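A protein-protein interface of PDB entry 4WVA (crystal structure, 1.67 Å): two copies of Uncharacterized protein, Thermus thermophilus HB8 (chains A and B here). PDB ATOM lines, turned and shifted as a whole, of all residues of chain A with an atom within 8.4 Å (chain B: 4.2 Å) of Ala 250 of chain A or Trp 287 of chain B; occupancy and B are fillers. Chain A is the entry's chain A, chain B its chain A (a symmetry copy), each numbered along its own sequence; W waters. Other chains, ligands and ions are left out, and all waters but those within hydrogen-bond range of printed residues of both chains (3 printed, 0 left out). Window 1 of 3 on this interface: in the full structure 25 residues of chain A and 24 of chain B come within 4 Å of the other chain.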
ATOM      1  N   ALA A 108      15.696   3.835 -24.911  1.00  0.00           N
ATOM      2  CA  ALA A 108      14.296   3.890 -24.407  1.00  0.00           C
ATOM      3  C   ALA A 108      14.222   4.290 -22.944  1.00  0.00           C
ATOM      4  O   ALA A 108      13.280   4.945 -22.503  1.00  0.00           O
ATOM      5  CB  ALA A 108      13.581   2.569 -24.623  1.00  0.00           C
ATOM      6  N   ARG A 112      12.150   7.465 -21.616  1.00  0.00           N
ATOM      7  CA  ARG A 112      11.148   7.399 -20.544  1.00  0.00           C
ATOM      8  C   ARG A 112      11.425   8.496 -19.504  1.00  0.00           C
ATOM      9  O   ARG A 112      10.517   9.186 -19.036  1.00  0.00           O
ATOM     10  CB  ARG A 112      11.127   6.030 -19.871  1.00  0.00           C
ATOM     11  CG  ARG A 112      10.132   5.995 -18.719  1.00  0.00           C
ATOM     12  CD  ARG A 112      10.125   4.663 -17.992  1.00  0.00           C
ATOM     13  NE  ARG A 112       9.162   4.690 -16.888  1.00  0.00           N
ATOM     14  CZ  ARG A 112       8.925   3.667 -16.063  1.00  0.00           C
ATOM     15  NH1 ARG A 112       9.571   2.526 -16.190  1.00  0.00           N
ATOM     16  NH2 ARG A 112       8.031   3.801 -15.086  1.00  0.00           N
ATOM     17  N   TYR A 115      10.570  11.857 -20.911  1.00  0.00           N
ATOM     18  CA  TYR A 115       9.120  11.957 -21.008  1.00  0.00           C
ATOM     19  C   TYR A 115       8.468  12.266 -19.661  1.00  0.00           C
ATOM     20  O   TYR A 115       7.606  13.142 -19.555  1.00  0.00           O
ATOM     21  CB  TYR A 115       8.495  10.695 -21.633  1.00  0.00           C
ATOM     22  CG  TYR A 115       6.994  10.775 -21.614  1.00  0.00           C
ATOM     23  CD1 TYR A 115       6.330  11.736 -22.375  1.00  0.00           C
ATOM     24  CD2 TYR A 115       6.232   9.954 -20.795  1.00  0.00           C
ATOM     25  CE1 TYR A 115       4.959  11.833 -22.361  1.00  0.00           C
ATOM     26  CE2 TYR A 115       4.851  10.055 -20.762  1.00  0.00           C
ATOM     27  CZ  TYR A 115       4.213  11.003 -21.553  1.00  0.00           C
ATOM     28  OH  TYR A 115       2.837  11.137 -21.552  1.00  0.00           O
ATOM     29  N   GLU A 116       8.901  11.564 -18.620  1.00  0.00           N
ATOM     30  CA  GLU A 116       8.243  11.681 -17.315  1.00  0.00           C
ATOM     31  C   GLU A 116       8.633  12.965 -16.590  1.00  0.00           C
ATOM     32  O   GLU A 116       7.837  13.495 -15.795  1.00  0.00           O
ATOM     33  CB  GLU A 116       8.566  10.470 -16.433  1.00  0.00           C
ATOM     34  CG  GLU A 116       7.911   9.178 -16.917  1.00  0.00           C
ATOM     35  CD  GLU A 116       8.183   7.994 -16.013  1.00  0.00           C
ATOM     36  OE1 GLU A 116       9.000   8.140 -15.088  1.00  0.00           O
ATOM     37  OE2 GLU A 116       7.609   6.921 -16.231  1.00  0.00           O
ATOM     38  N   PHE A 132       8.274   7.092 -29.988  1.00  0.00           N
ATOM     39  CA  PHE A 132       7.843   5.769 -29.574  1.00  0.00           C
ATOM     40  C   PHE A 132       7.854   4.720 -30.716  1.00  0.00           C
ATOM     41  O   PHE A 132       8.416   3.633 -30.550  1.00  0.00           O
ATOM     42  CB  PHE A 132       6.465   5.800 -28.905  1.00  0.00           C
ATOM     43  CG  PHE A 132       5.974   4.438 -28.537  1.00  0.00           C
ATOM     44  CD1 PHE A 132       6.438   3.807 -27.400  1.00  0.00           C
ATOM     45  CD2 PHE A 132       5.098   3.762 -29.367  1.00  0.00           C
ATOM     46  CE1 PHE A 132       6.012   2.528 -27.081  1.00  0.00           C
ATOM     47  CE2 PHE A 132       4.669   2.482 -29.068  1.00  0.00           C
ATOM     48  CZ  PHE A 132       5.136   1.861 -27.921  1.00  0.00           C
ATOM     49  N   ARG A 243      16.338  -3.721 -19.619  1.00  0.00           N
ATOM     50  CA  ARG A 243      15.928  -2.483 -18.960  1.00  0.00           C
ATOM     51  C   ARG A 243      15.152  -1.587 -19.923  1.00  0.00           C
ATOM     52  O   ARG A 243      14.099  -1.044 -19.562  1.00  0.00           O
ATOM     53  CB  ARG A 243      17.123  -1.742 -18.372  1.00  0.00           C
ATOM     54  CG  ARG A 243      16.790  -0.393 -17.755  1.00  0.00           C
ATOM     55  CD  ARG A 243      15.735  -0.422 -16.663  1.00  0.00           C
ATOM     56  NE  ARG A 243      15.502   0.921 -16.142  1.00  0.00           N
ATOM     57  CZ  ARG A 243      16.198   1.491 -15.146  1.00  0.00           C
ATOM     58  NH1 ARG A 243      17.155   0.841 -14.521  1.00  0.00           N
ATOM     59  NH2 ARG A 243      15.918   2.726 -14.769  1.00  0.00           N
ATOM     60  N   ALA A 244      15.654  -1.457 -21.148  1.00  0.00           N
ATOM     61  CA  ALA A 244      15.031  -0.600 -22.128  1.00  0.00           C
ATOM     62  C   ALA A 244      13.635  -1.109 -22.503  1.00  0.00           C
ATOM     63  O   ALA A 244      12.731  -0.305 -22.684  1.00  0.00           O
ATOM     64  CB  ALA A 244      15.919  -0.465 -23.347  1.00  0.00           C
ATOM     65  N   ASN A 245      13.470  -2.426 -22.628  1.00  0.00           N
ATOM     66  CA  ASN A 245      12.139  -3.026 -22.857  1.00  0.00           C
ATOM     67  C   ASN A 245      11.146  -2.697 -21.739  1.00  0.00           C
ATOM     68  O   ASN A 245       9.996  -2.322 -22.012  1.00  0.00           O
ATOM     69  CB  ASN A 245      12.206  -4.545 -23.003  1.00  0.00           C
ATOM     70  CG  ASN A 245      12.736  -4.996 -24.351  1.00  0.00           C
ATOM     71  OD1 ASN A 245      12.506  -4.350 -25.367  1.00  0.00           O
ATOM     72  ND2 ASN A 245      13.423  -6.119 -24.369  1.00  0.00           N
ATOM     73  N   ARG A 246      11.579  -2.817 -20.491  1.00  0.00           N
ATOM     74  CA  ARG A 246      10.729  -2.449 -19.366  1.00  0.00           C
ATOM     75  C   ARG A 246      10.297  -0.988 -19.448  1.00  0.00           C
ATOM     76  O   ARG A 246       9.131  -0.636 -19.181  1.00  0.00           O
ATOM     77  CB  ARG A 246      11.466  -2.677 -18.036  1.00  0.00           C
ATOM     78  CG  ARG A 246      11.797  -4.128 -17.778  1.00  0.00           C
ATOM     79  CD  ARG A 246      10.772  -4.824 -16.951  1.00  0.00           C
ATOM     80  NE  ARG A 246      11.172  -6.206 -16.649  1.00  0.00           N
ATOM     81  CZ  ARG A 246      10.392  -7.051 -15.997  1.00  0.00           C
ATOM     82  NH1 ARG A 246       9.196  -6.646 -15.560  1.00  0.00           N
ATOM     83  NH2 ARG A 246      10.799  -8.306 -15.784  1.00  0.00           N
ATOM     84  N   ASP A 247      11.236  -0.117 -19.801  1.00  0.00           N
ATOM     85  CA  ASP A 247      10.929   1.297 -19.905  1.00  0.00           C
ATOM     86  C   ASP A 247      10.069   1.639 -21.137  1.00  0.00           C
ATOM     87  O   ASP A 247       9.202   2.525 -21.056  1.00  0.00           O
ATOM     88  CB  ASP A 247      12.212   2.122 -19.844  1.00  0.00           C
ATOM     89  CG  ASP A 247      12.877   2.044 -18.485  1.00  0.00           C
ATOM     90  OD1 ASP A 247      12.132   1.910 -17.491  1.00  0.00           O
ATOM     91  OD2 ASP A 247      14.111   2.059 -18.411  1.00  0.00           O
ATOM     92  N   LEU A 248      10.285   0.933 -22.243  1.00  0.00           N
ATOM     93  CA  LEU A 248       9.458   1.075 -23.429  1.00  0.00           C
ATOM     94  C   LEU A 248       8.009   0.649 -23.179  1.00  0.00           C
ATOM     95  O   LEU A 248       7.075   1.287 -23.674  1.00  0.00           O
ATOM     96  CB  LEU A 248      10.044   0.299 -24.606  1.00  0.00           C
ATOM     97  CG  LEU A 248       9.424   0.587 -25.971  1.00  0.00           C
ATOM     98  CD1 LEU A 248       9.652   2.036 -26.389  1.00  0.00           C
ATOM     99  CD2 LEU A 248      10.004  -0.372 -26.991  1.00  0.00           C
ATOM    100  N   TYR A 249       7.841  -0.432 -22.412  1.00  0.00           N
ATOM    101  CA  TYR A 249       6.524  -0.882 -21.971  1.00  0.00           C
ATOM    102  C   TYR A 249       5.797   0.250 -21.230  1.00  0.00           C
ATOM    103  O   TYR A 249       4.637   0.560 -21.500  1.00  0.00           O
ATOM    104  CB  TYR A 249       6.654  -2.116 -21.068  1.00  0.00           C
ATOM    105  CG  TYR A 249       5.353  -2.417 -20.346  1.00  0.00           C
ATOM    106  CD1 TYR A 249       4.381  -3.220 -20.937  1.00  0.00           C
ATOM    107  CD2 TYR A 249       5.082  -1.870 -19.103  1.00  0.00           C
ATOM    108  CE1 TYR A 249       3.170  -3.466 -20.309  1.00  0.00           C
ATOM    109  CE2 TYR A 249       3.869  -2.108 -18.465  1.00  0.00           C
ATOM    110  CZ  TYR A 249       2.924  -2.905 -19.074  1.00  0.00           C
ATOM    111  OH  TYR A 249       1.721  -3.130 -18.422  1.00  0.00           O
ATOM    112  N   ALA A 250       6.489   0.875 -20.281  1.00  0.00           N
ATOM    113  CA  ALA A 250       5.881   1.938 -19.492  1.00  0.00           C
ATOM    114  C   ALA A 250       5.453   3.093 -20.378  1.00  0.00           C
ATOM    115  O   ALA A 250       4.340   3.596 -20.264  1.00  0.00           O
ATOM    116  CB  ALA A 250       6.836   2.404 -18.396  1.00  0.00           C
ATOM    117  N   LEU A 251       6.331   3.495 -21.291  1.00  0.00           N
ATOM    118  CA  LEU A 251       5.970   4.517 -22.311  1.00  0.00           C
ATOM    119  C   LEU A 251       4.741   4.130 -23.112  1.00  0.00           C
ATOM    120  O   LEU A 251       3.850   4.953 -23.291  1.00  0.00           O
ATOM    121  CB  LEU A 251       7.129   4.770 -23.270  1.00  0.00           C
ATOM    122  CG  LEU A 251       8.239   5.653 -22.759  1.00  0.00           C
ATOM    123  CD1 LEU A 251       9.493   5.451 -23.601  1.00  0.00           C
ATOM    124  CD2 LEU A 251       7.788   7.115 -22.754  1.00  0.00           C
ATOM    125  N   ALA A 252       4.690   2.892 -23.592  1.00  0.00           N
ATOM    126  CA  ALA A 252       3.537   2.406 -24.348  1.00  0.00           C
ATOM    127  C   ALA A 252       2.243   2.572 -23.556  1.00  0.00           C
ATOM    128  O   ALA A 252       1.235   3.064 -24.081  1.00  0.00           O
ATOM    129  CB  ALA A 252       3.720   0.950 -24.735  1.00  0.00           C
ATOM    130  N   VAL A 253       2.262   2.149 -22.297  1.00  0.00           N
ATOM    131  CA  VAL A 253       1.039   2.230 -21.489  1.00  0.00           C
ATOM    132  C   VAL A 253       0.654   3.692 -21.270  1.00  0.00           C
ATOM    133  O   VAL A 253      -0.532   4.049 -21.410  1.00  0.00           O
ATOM    134  CB  VAL A 253       1.152   1.482 -20.140  1.00  0.00           C
ATOM    135  CG1 VAL A 253      -0.118   1.667 -19.327  1.00  0.00           C
ATOM    136  CG2 VAL A 253       1.380  -0.002 -20.375  1.00  0.00           C
ATOM    137  N   LEU A 254       1.625   4.524 -20.907  1.00  0.00           N
ATOM    138  CA  LEU A 254       1.365   5.949 -20.658  1.00  0.00           C
ATOM    139  C   LEU A 254       0.827   6.683 -21.885  1.00  0.00           C
ATOM    140  O   LEU A 254      -0.046   7.553 -21.752  1.00  0.00           O
ATOM    141  CB  LEU A 254       2.605   6.641 -20.112  1.00  0.00           C
ATOM    142  CG  LEU A 254       3.008   6.224 -18.689  1.00  0.00           C
ATOM    143  CD1 LEU A 254       4.379   6.728 -18.353  1.00  0.00           C
ATOM    144  CD2 LEU A 254       2.000   6.739 -17.663  1.00  0.00           C
ATOM    145  N   LEU A 255       1.319   6.299 -23.052  1.00  0.00           N
ATOM    146  CA  LEU A 255       0.891   6.880 -24.344  1.00  0.00           C
ATOM    147  C   LEU A 255      -0.343   6.186 -24.939  1.00  0.00           C
ATOM    148  O   LEU A 255      -0.844   6.577 -26.007  1.00  0.00           O
ATOM    149  CB  LEU A 255       2.040   6.823 -25.354  1.00  0.00           C
ATOM    150  CG  LEU A 255       3.296   7.628 -25.057  1.00  0.00           C
ATOM    151  CD1 LEU A 255       4.310   7.371 -26.161  1.00  0.00           C
ATOM    152  CD2 LEU A 255       3.027   9.113 -24.891  1.00  0.00           C
ATOM    153  N   GLN A 256      -0.831   5.156 -24.263  1.00  0.00           N
ATOM    154  CA  GLN A 256      -1.988   4.385 -24.705  1.00  0.00           C
ATOM    155  C   GLN A 256      -1.771   3.732 -26.069  1.00  0.00           C
ATOM    156  O   GLN A 256      -2.605   3.839 -26.975  1.00  0.00           O
ATOM    157  CB  GLN A 256      -3.285   5.217 -24.603  1.00  0.00           C
ATOM    158  CG  GLN A 256      -3.647   5.539 -23.149  1.00  0.00           C
ATOM    159  CD  GLN A 256      -4.260   4.352 -22.431  1.00  0.00           C
ATOM    160  OE1 GLN A 256      -5.485   4.143 -22.473  1.00  0.00           O
ATOM    161  NE2 GLN A 256      -3.422   3.549 -21.778  1.00  0.00           N
ATOM    162  N   GLU A 257      -0.631   3.046 -26.179  1.00  0.00           N
ATOM    163  CA  GLU A 257      -0.321   2.151 -27.287  1.00  0.00           C
ATOM    164  C   GLU A 257      -0.354   0.703 -26.775  1.00  0.00           C
ATOM    165  O   GLU A 257      -0.238   0.469 -25.577  1.00  0.00           O
ATOM    166  CB  GLU A 257       1.056   2.486 -27.856  1.00  0.00           C
ATOM    167  CG  GLU A 257       1.145   3.882 -28.438  1.00  0.00           C
ATOM    168  CD  GLU A 257       0.352   4.015 -29.730  1.00  0.00           C
ATOM    169  OE1 GLU A 257      -0.089   2.979 -30.265  1.00  0.00           O
ATOM    170  OE2 GLU A 257       0.144   5.150 -30.189  1.00  0.00           O
ATOM    171  N   PRO A 259       1.092  -2.654 -25.845  1.00  0.00           N
ATOM    172  CA  PRO A 259       2.447  -3.141 -25.588  1.00  0.00           C
ATOM    173  C   PRO A 259       2.593  -4.667 -25.590  1.00  0.00           C
ATOM    174  O   PRO A 259       3.565  -5.177 -25.046  1.00  0.00           O
ATOM    175  CB  PRO A 259       2.729  -2.623 -24.163  1.00  0.00           C
ATOM    176  CG  PRO A 259       1.389  -2.477 -23.534  1.00  0.00           C
ATOM    177  CD  PRO A 259       0.319  -2.590 -24.591  1.00  0.00           C
ATOM    178  N   ILE A 262       5.911  -5.980 -26.708  1.00  0.00           N
ATOM    179  CA  ILE A 262       6.973  -5.634 -25.755  1.00  0.00           C
ATOM    180  C   ILE A 262       6.923  -6.557 -24.527  1.00  0.00           C
ATOM    181  O   ILE A 262       7.955  -6.967 -24.003  1.00  0.00           O
ATOM    182  CB  ILE A 262       6.845  -4.168 -25.296  1.00  0.00           C
ATOM    183  CG1 ILE A 262       6.831  -3.200 -26.482  1.00  0.00           C
ATOM    184  CG2 ILE A 262       8.007  -3.800 -24.379  1.00  0.00           C
ATOM    185  CD1 ILE A 262       6.320  -1.820 -26.113  1.00  0.00           C
ATOM    186  N   ILE A 266       9.978  -8.754 -22.845  1.00  0.00           N
ATOM    187  CA  ILE A 266      10.339  -8.623 -21.433  1.00  0.00           C
ATOM    188  C   ILE A 266      10.382 -10.000 -20.742  1.00  0.00           C
ATOM    189  O   ILE A 266      11.328 -10.329 -20.028  1.00  0.00           O
ATOM    190  CB  ILE A 266       9.337  -7.690 -20.719  1.00  0.00           C
ATOM    191  CG1 ILE A 266       9.527  -6.244 -21.207  1.00  0.00           C
ATOM    192  CG2 ILE A 266       9.509  -7.786 -19.215  1.00  0.00           C
ATOM    193  CD1 ILE A 266       8.476  -5.267 -20.739  1.00  0.00           C
ATOM    194  N   VAL B 232      -7.553   5.947 -14.942  1.00  0.00           N
ATOM    195  CA  VAL B 232      -6.404   5.831 -14.076  1.00  0.00           C
ATOM    196  C   VAL B 232      -6.015   4.368 -13.906  1.00  0.00           C
ATOM    197  O   VAL B 232      -6.892   3.502 -13.771  1.00  0.00           O
ATOM    198  CB  VAL B 232      -6.736   6.437 -12.701  1.00  0.00           C
ATOM    199  CG1 VAL B 232      -5.696   6.084 -11.664  1.00  0.00           C
ATOM    200  CG2 VAL B 232      -6.858   7.942 -12.837  1.00  0.00           C
ATOM    201  N   VAL B 233      -4.709   4.098 -13.947  1.00  0.00           N
ATOM    202  CA  VAL B 233      -4.187   2.814 -13.498  1.00  0.00           C
ATOM    203  C   VAL B 233      -3.877   2.979 -12.011  1.00  0.00           C
ATOM    204  O   VAL B 233      -2.882   3.593 -11.627  1.00  0.00           O
ATOM    205  CB  VAL B 233      -2.939   2.354 -14.285  1.00  0.00           C
ATOM    206  CG1 VAL B 233      -2.375   1.075 -13.672  1.00  0.00           C
ATOM    207  CG2 VAL B 233      -3.297   2.146 -15.757  1.00  0.00           C
ATOM    208  N   ALA B 275       6.025  -1.987 -13.392  1.00  0.00           N
ATOM    209  CA  ALA B 275       6.240  -0.766 -14.150  1.00  0.00           C
ATOM    210  C   ALA B 275       5.854   0.481 -13.355  1.00  0.00           C
ATOM    211  O   ALA B 275       6.376   1.552 -13.605  1.00  0.00           O
ATOM    212  CB  ALA B 275       5.470  -0.796 -15.462  1.00  0.00           C
ATOM    213  N   LEU B 276       4.932   0.350 -12.411  1.00  0.00           N
ATOM    214  CA  LEU B 276       4.457   1.503 -11.642  1.00  0.00           C
ATOM    215  C   LEU B 276       5.479   2.013 -10.649  1.00  0.00           C
ATOM    216  O   LEU B 276       5.311   3.095 -10.067  1.00  0.00           O
ATOM    217  CB  LEU B 276       3.159   1.156 -10.905  1.00  0.00           C
ATOM    218  CG  LEU B 276       1.993   0.660 -11.781  1.00  0.00           C
ATOM    219  CD1 LEU B 276       0.783   0.377 -10.912  1.00  0.00           C
ATOM    220  CD2 LEU B 276       1.661   1.670 -12.861  1.00  0.00           C
ATOM    221  N   PHE B 285       3.588   4.396  -7.908  1.00  0.00           N
ATOM    222  CA  PHE B 285       2.585   5.416  -8.216  1.00  0.00           C
ATOM    223  C   PHE B 285       1.475   4.851  -9.079  1.00  0.00           C
ATOM    224  O   PHE B 285       1.715   4.025  -9.956  1.00  0.00           O
ATOM    225  CB  PHE B 285       3.210   6.581  -8.996  1.00  0.00           C
ATOM    226  CG  PHE B 285       4.153   7.445  -8.189  1.00  0.00           C
ATOM    227  CD1 PHE B 285       3.914   7.728  -6.858  1.00  0.00           C
ATOM    228  CD2 PHE B 285       5.271   8.015  -8.800  1.00  0.00           C
ATOM    229  CE1 PHE B 285       4.786   8.541  -6.133  1.00  0.00           C
ATOM    230  CE2 PHE B 285       6.142   8.824  -8.079  1.00  0.00           C
ATOM    231  CZ  PHE B 285       5.899   9.073  -6.745  1.00  0.00           C
ATOM    232  N   SER B 286       0.260   5.357  -8.865  1.00  0.00           N
ATOM    233  CA  SER B 286      -0.793   5.199  -9.847  1.00  0.00           C
ATOM    234  C   SER B 286      -0.472   6.092 -11.059  1.00  0.00           C
ATOM    235  O   SER B 286       0.318   7.047 -10.948  1.00  0.00           O
ATOM    236  CB  SER B 286      -2.136   5.590  -9.231  1.00  0.00           C
ATOM    237  OG  SER B 286      -2.486   4.731  -8.149  1.00  0.00           O
ATOM    238  N   TRP B 287      -1.068   5.753 -12.205  1.00  0.00           N
ATOM    239  CA  TRP B 287      -0.871   6.474 -13.447  1.00  0.00           C
ATOM    240  C   TRP B 287      -2.155   7.095 -13.979  1.00  0.00           C
ATOM    241  O   TRP B 287      -3.219   6.480 -13.961  1.00  0.00           O
ATOM    242  CB  TRP B 287      -0.282   5.564 -14.509  1.00  0.00           C
ATOM    243  CG  TRP B 287       1.126   5.132 -14.299  1.00  0.00           C
ATOM    244  CD1 TRP B 287       1.997   5.529 -13.327  1.00  0.00           C
ATOM    245  CD2 TRP B 287       1.849   4.234 -15.137  1.00  0.00           C
ATOM    246  NE1 TRP B 287       3.214   4.920 -13.511  1.00  0.00           N
ATOM    247  CE2 TRP B 287       3.143   4.123 -14.615  1.00  0.00           C
ATOM    248  CE3 TRP B 287       1.511   3.490 -16.273  1.00  0.00           C
ATOM    249  CZ2 TRP B 287       4.113   3.308 -15.198  1.00  0.00           C
ATOM    250  CZ3 TRP B 287       2.476   2.683 -16.845  1.00  0.00           C
ATOM    251  CH2 TRP B 287       3.756   2.596 -16.300  1.00  0.00           C
ATOM    252  N   ASP B 288      -2.023   8.319 -14.482  1.00  0.00           N
ATOM    253  CA  ASP B 288      -3.123   9.047 -15.092  1.00  0.00           C
ATOM    254  C   ASP B 288      -3.012   8.894 -16.593  1.00  0.00           C
ATOM    255  O   ASP B 288      -2.090   9.445 -17.205  1.00  0.00           O
ATOM    256  CB  ASP B 288      -3.019  10.522 -14.691  1.00  0.00           C
ATOM    257  CG  ASP B 288      -4.068  11.397 -15.343  1.00  0.00           C
ATOM    258  OD1 ASP B 288      -4.767  10.947 -16.272  1.00  0.00           O
ATOM    259  OD2 ASP B 288      -4.132  12.577 -14.913  1.00  0.00           O
ATOM    260  N   LEU B 289      -3.934   8.149 -17.179  1.00  0.00           N
ATOM    261  CA  LEU B 289      -3.843   7.823 -18.612  1.00  0.00           C
ATOM    262  C   LEU B 289      -4.426   8.906 -19.503  1.00  0.00           C
ATOM    263  O   LEU B 289      -4.192   8.890 -20.717  1.00  0.00           O
ATOM    264  CB  LEU B 289      -4.487   6.491 -18.931  1.00  0.00           C
ATOM    265  CG  LEU B 289      -3.881   5.239 -18.276  1.00  0.00           C
ATOM    266  CD1 LEU B 289      -4.595   4.005 -18.794  1.00  0.00           C
ATOM    267  CD2 LEU B 289      -2.392   5.117 -18.500  1.00  0.00           C
ATOM    268  N   GLU B 293       0.672  10.333 -17.559  1.00  0.00           N
ATOM    269  CA  GLU B 293       1.717  10.628 -16.576  1.00  0.00           C
ATOM    270  C   GLU B 293       1.546   9.835 -15.302  1.00  0.00           C
ATOM    271  O   GLU B 293       0.418   9.666 -14.835  1.00  0.00           O
ATOM    272  CB  GLU B 293       1.618  12.082 -16.124  1.00  0.00           C
ATOM    273  CG  GLU B 293       1.816  13.080 -17.221  1.00  0.00           C
ATOM    274  CD  GLU B 293       1.594  14.498 -16.748  1.00  0.00           C
ATOM    275  OE1 GLU B 293       1.282  14.735 -15.551  1.00  0.00           O
ATOM    276  OE2 GLU B 293       1.730  15.387 -17.596  1.00  0.00           O
ATOM    277  N   PRO B 294       2.658   9.443 -14.671  1.00  0.00           N
ATOM    278  CA  PRO B 294       2.526   9.010 -13.281  1.00  0.00           C
ATOM    279  C   PRO B 294       1.962  10.100 -12.372  1.00  0.00           C
ATOM    280  O   PRO B 294       2.238  11.284 -12.557  1.00  0.00           O
ATOM    281  CB  PRO B 294       3.962   8.659 -12.885  1.00  0.00           C
ATOM    282  CG  PRO B 294       4.633   8.354 -14.177  1.00  0.00           C
ATOM    283  CD  PRO B 294       4.046   9.347 -15.142  1.00  0.00           C
ATOM    284  N   ILE B 295       1.158   9.692 -11.398  1.00  0.00           N
ATOM    285  CA  ILE B 295       0.648  10.583 -10.380  1.00  0.00           C
ATOM    286  C   ILE B 295       1.610  10.525  -9.194  1.00  0.00           C
ATOM    287  O   ILE B 295       1.646   9.541  -8.438  1.00  0.00           O
ATOM    288  CB  ILE B 295      -0.762  10.162  -9.929  1.00  0.00           C
ATOM    289  CG1 ILE B 295      -1.747  10.158 -11.122  1.00  0.00           C
ATOM    290  CG2 ILE B 295      -1.235  11.074  -8.796  1.00  0.00           C
ATOM    291  CD1 ILE B 295      -3.009   9.359 -10.881  1.00  0.00           C
HETATM  292  O   HOH W   1       9.374   1.262 -13.380  1.00  0.00           O
HETATM  293  O   HOH W   2       2.245  13.981 -20.428  1.00  0.00           O
HETATM  294  O   HOH W   3      -2.127   8.949 -22.609  1.00  0.00           O
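NH2 of Arg 112 of chain A lies within hydrogen-bond range of O of Ala 275 of chain B (3.2 Å).
The side-chain carboxylate (OD1) of Asp 247 of chain A lies within salt-bridge range of the guanidinium group (NH1) of Arg 112 of chain A.
The backbone carbonyl oxygen (O) of Trp 287 of chain B lies within hydrogen-bond range of the backbone NH (N) of Val 233 of chain B (2.8 Å).
N of Asp 288 of chain B is in hydrogen-bond range of O of Glu 293 of chain B.
NE2 of Gln 256 of chain A lies within hydrogen-bond range of O of Val 253 of chain A (3.0 Å).
NE of Arg 112 of chain A lies within salt-bridge range of OE2 of Glu 116 of chain A, at 2.8 Å.
Arg 112 of chain A touches Trp 287 of chain B (NH2 to CZ2, 3.95 Å).
Glu 116 of chain A touches Pro 294 of chain B.
Ala 275 of chain B touches Tyr 249 of chain A (CB to CE2, 3.6 Å).
Ala 250 of chain A touches Trp 287 of chain B.
CZ3 of Trp 287 of chain B touches CG1 of Val 253 of chain A, at 3.7 Å.
Val 253 of chain A touches Leu 289 of chain B (O to CD2, 3.6 Å).
CD2 of Trp 287 of chain B touches CD2 of Leu 254 of chain A, at 3.6 Å.
Leu 254 of chain A touches Glu 293 of chain B.
Gln 256 of chain A touches Leu 289 of chain B (NE2 to CD1, 3.2 Å).
Of the printed residues of chain B, Glu 116 of chain A touches Pro 294 (3.9 Å).
Asp 247 of chain A touches none of the printed residues of chain B.
Printed residues of chain B within 4 Å of Tyr 249 of chain A: Ala 275 (3.6 Å).
Ala 250 of chain A touches just one residue of chain B: Trp 287.
Of the printed residues of chain B, Val 253 of chain A touches Trp 287 and Leu 289.
Ile 262 of chain A touches none of the printed residues of chain B.
Of chain A, only Arg 112 (3.95 Å), Ala 250 (3.7 Å), Val 253 (3.7 Å) and Leu 254 (3.6 Å) come within 4 Å of Trp 287 of chain B.
The nearest residue of chain A that does not touch Trp 287 of chain B is Glu 116 of chain A (5.1 Å).
The nearest printed residue of chain B that does not touch Leu 254 of chain A is Pro 294 of chain B (4.1 Å).
Of the 12 printed residues of chain B, 5 touch a printed residue of chain A.
Hydrophobic or aromatic side chains of chain B that line the printed part of chain A: Ala 275, Trp 287, Leu 289 and Pro 294.
Printed residues of chain A that touch a printed residue of chain B: Arg 112, Glu 116, Tyr 249, Ala 250, Val 253, Leu 254 and Gln 256.
Hydrophobic or aromatic side chains of chain A within 4 Å of the printed part of chain B: Tyr 249, Ala 250, Val 253 and Leu 254.
No position is printed for both chains.
Of the 10 pairs that touch across the chains among the printed residues, none has its exchanged pair printed and touching as well.
Water W3 bridges O of Leu 254 of chain A (2.6 Å) and O of Leu 289 of chain B (2.8 Å).
Water W1 bridges the backbone carbonyl oxygen (O) of Ala 275 of chain B (3.0 Å) and the guanidinium group (NH1) of Arg 112 of chain A (3.1 Å).
Water W2 lies within hydrogen-bond range of OH of Tyr 115 of chain A and OE2 of Glu 293 of chain B.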
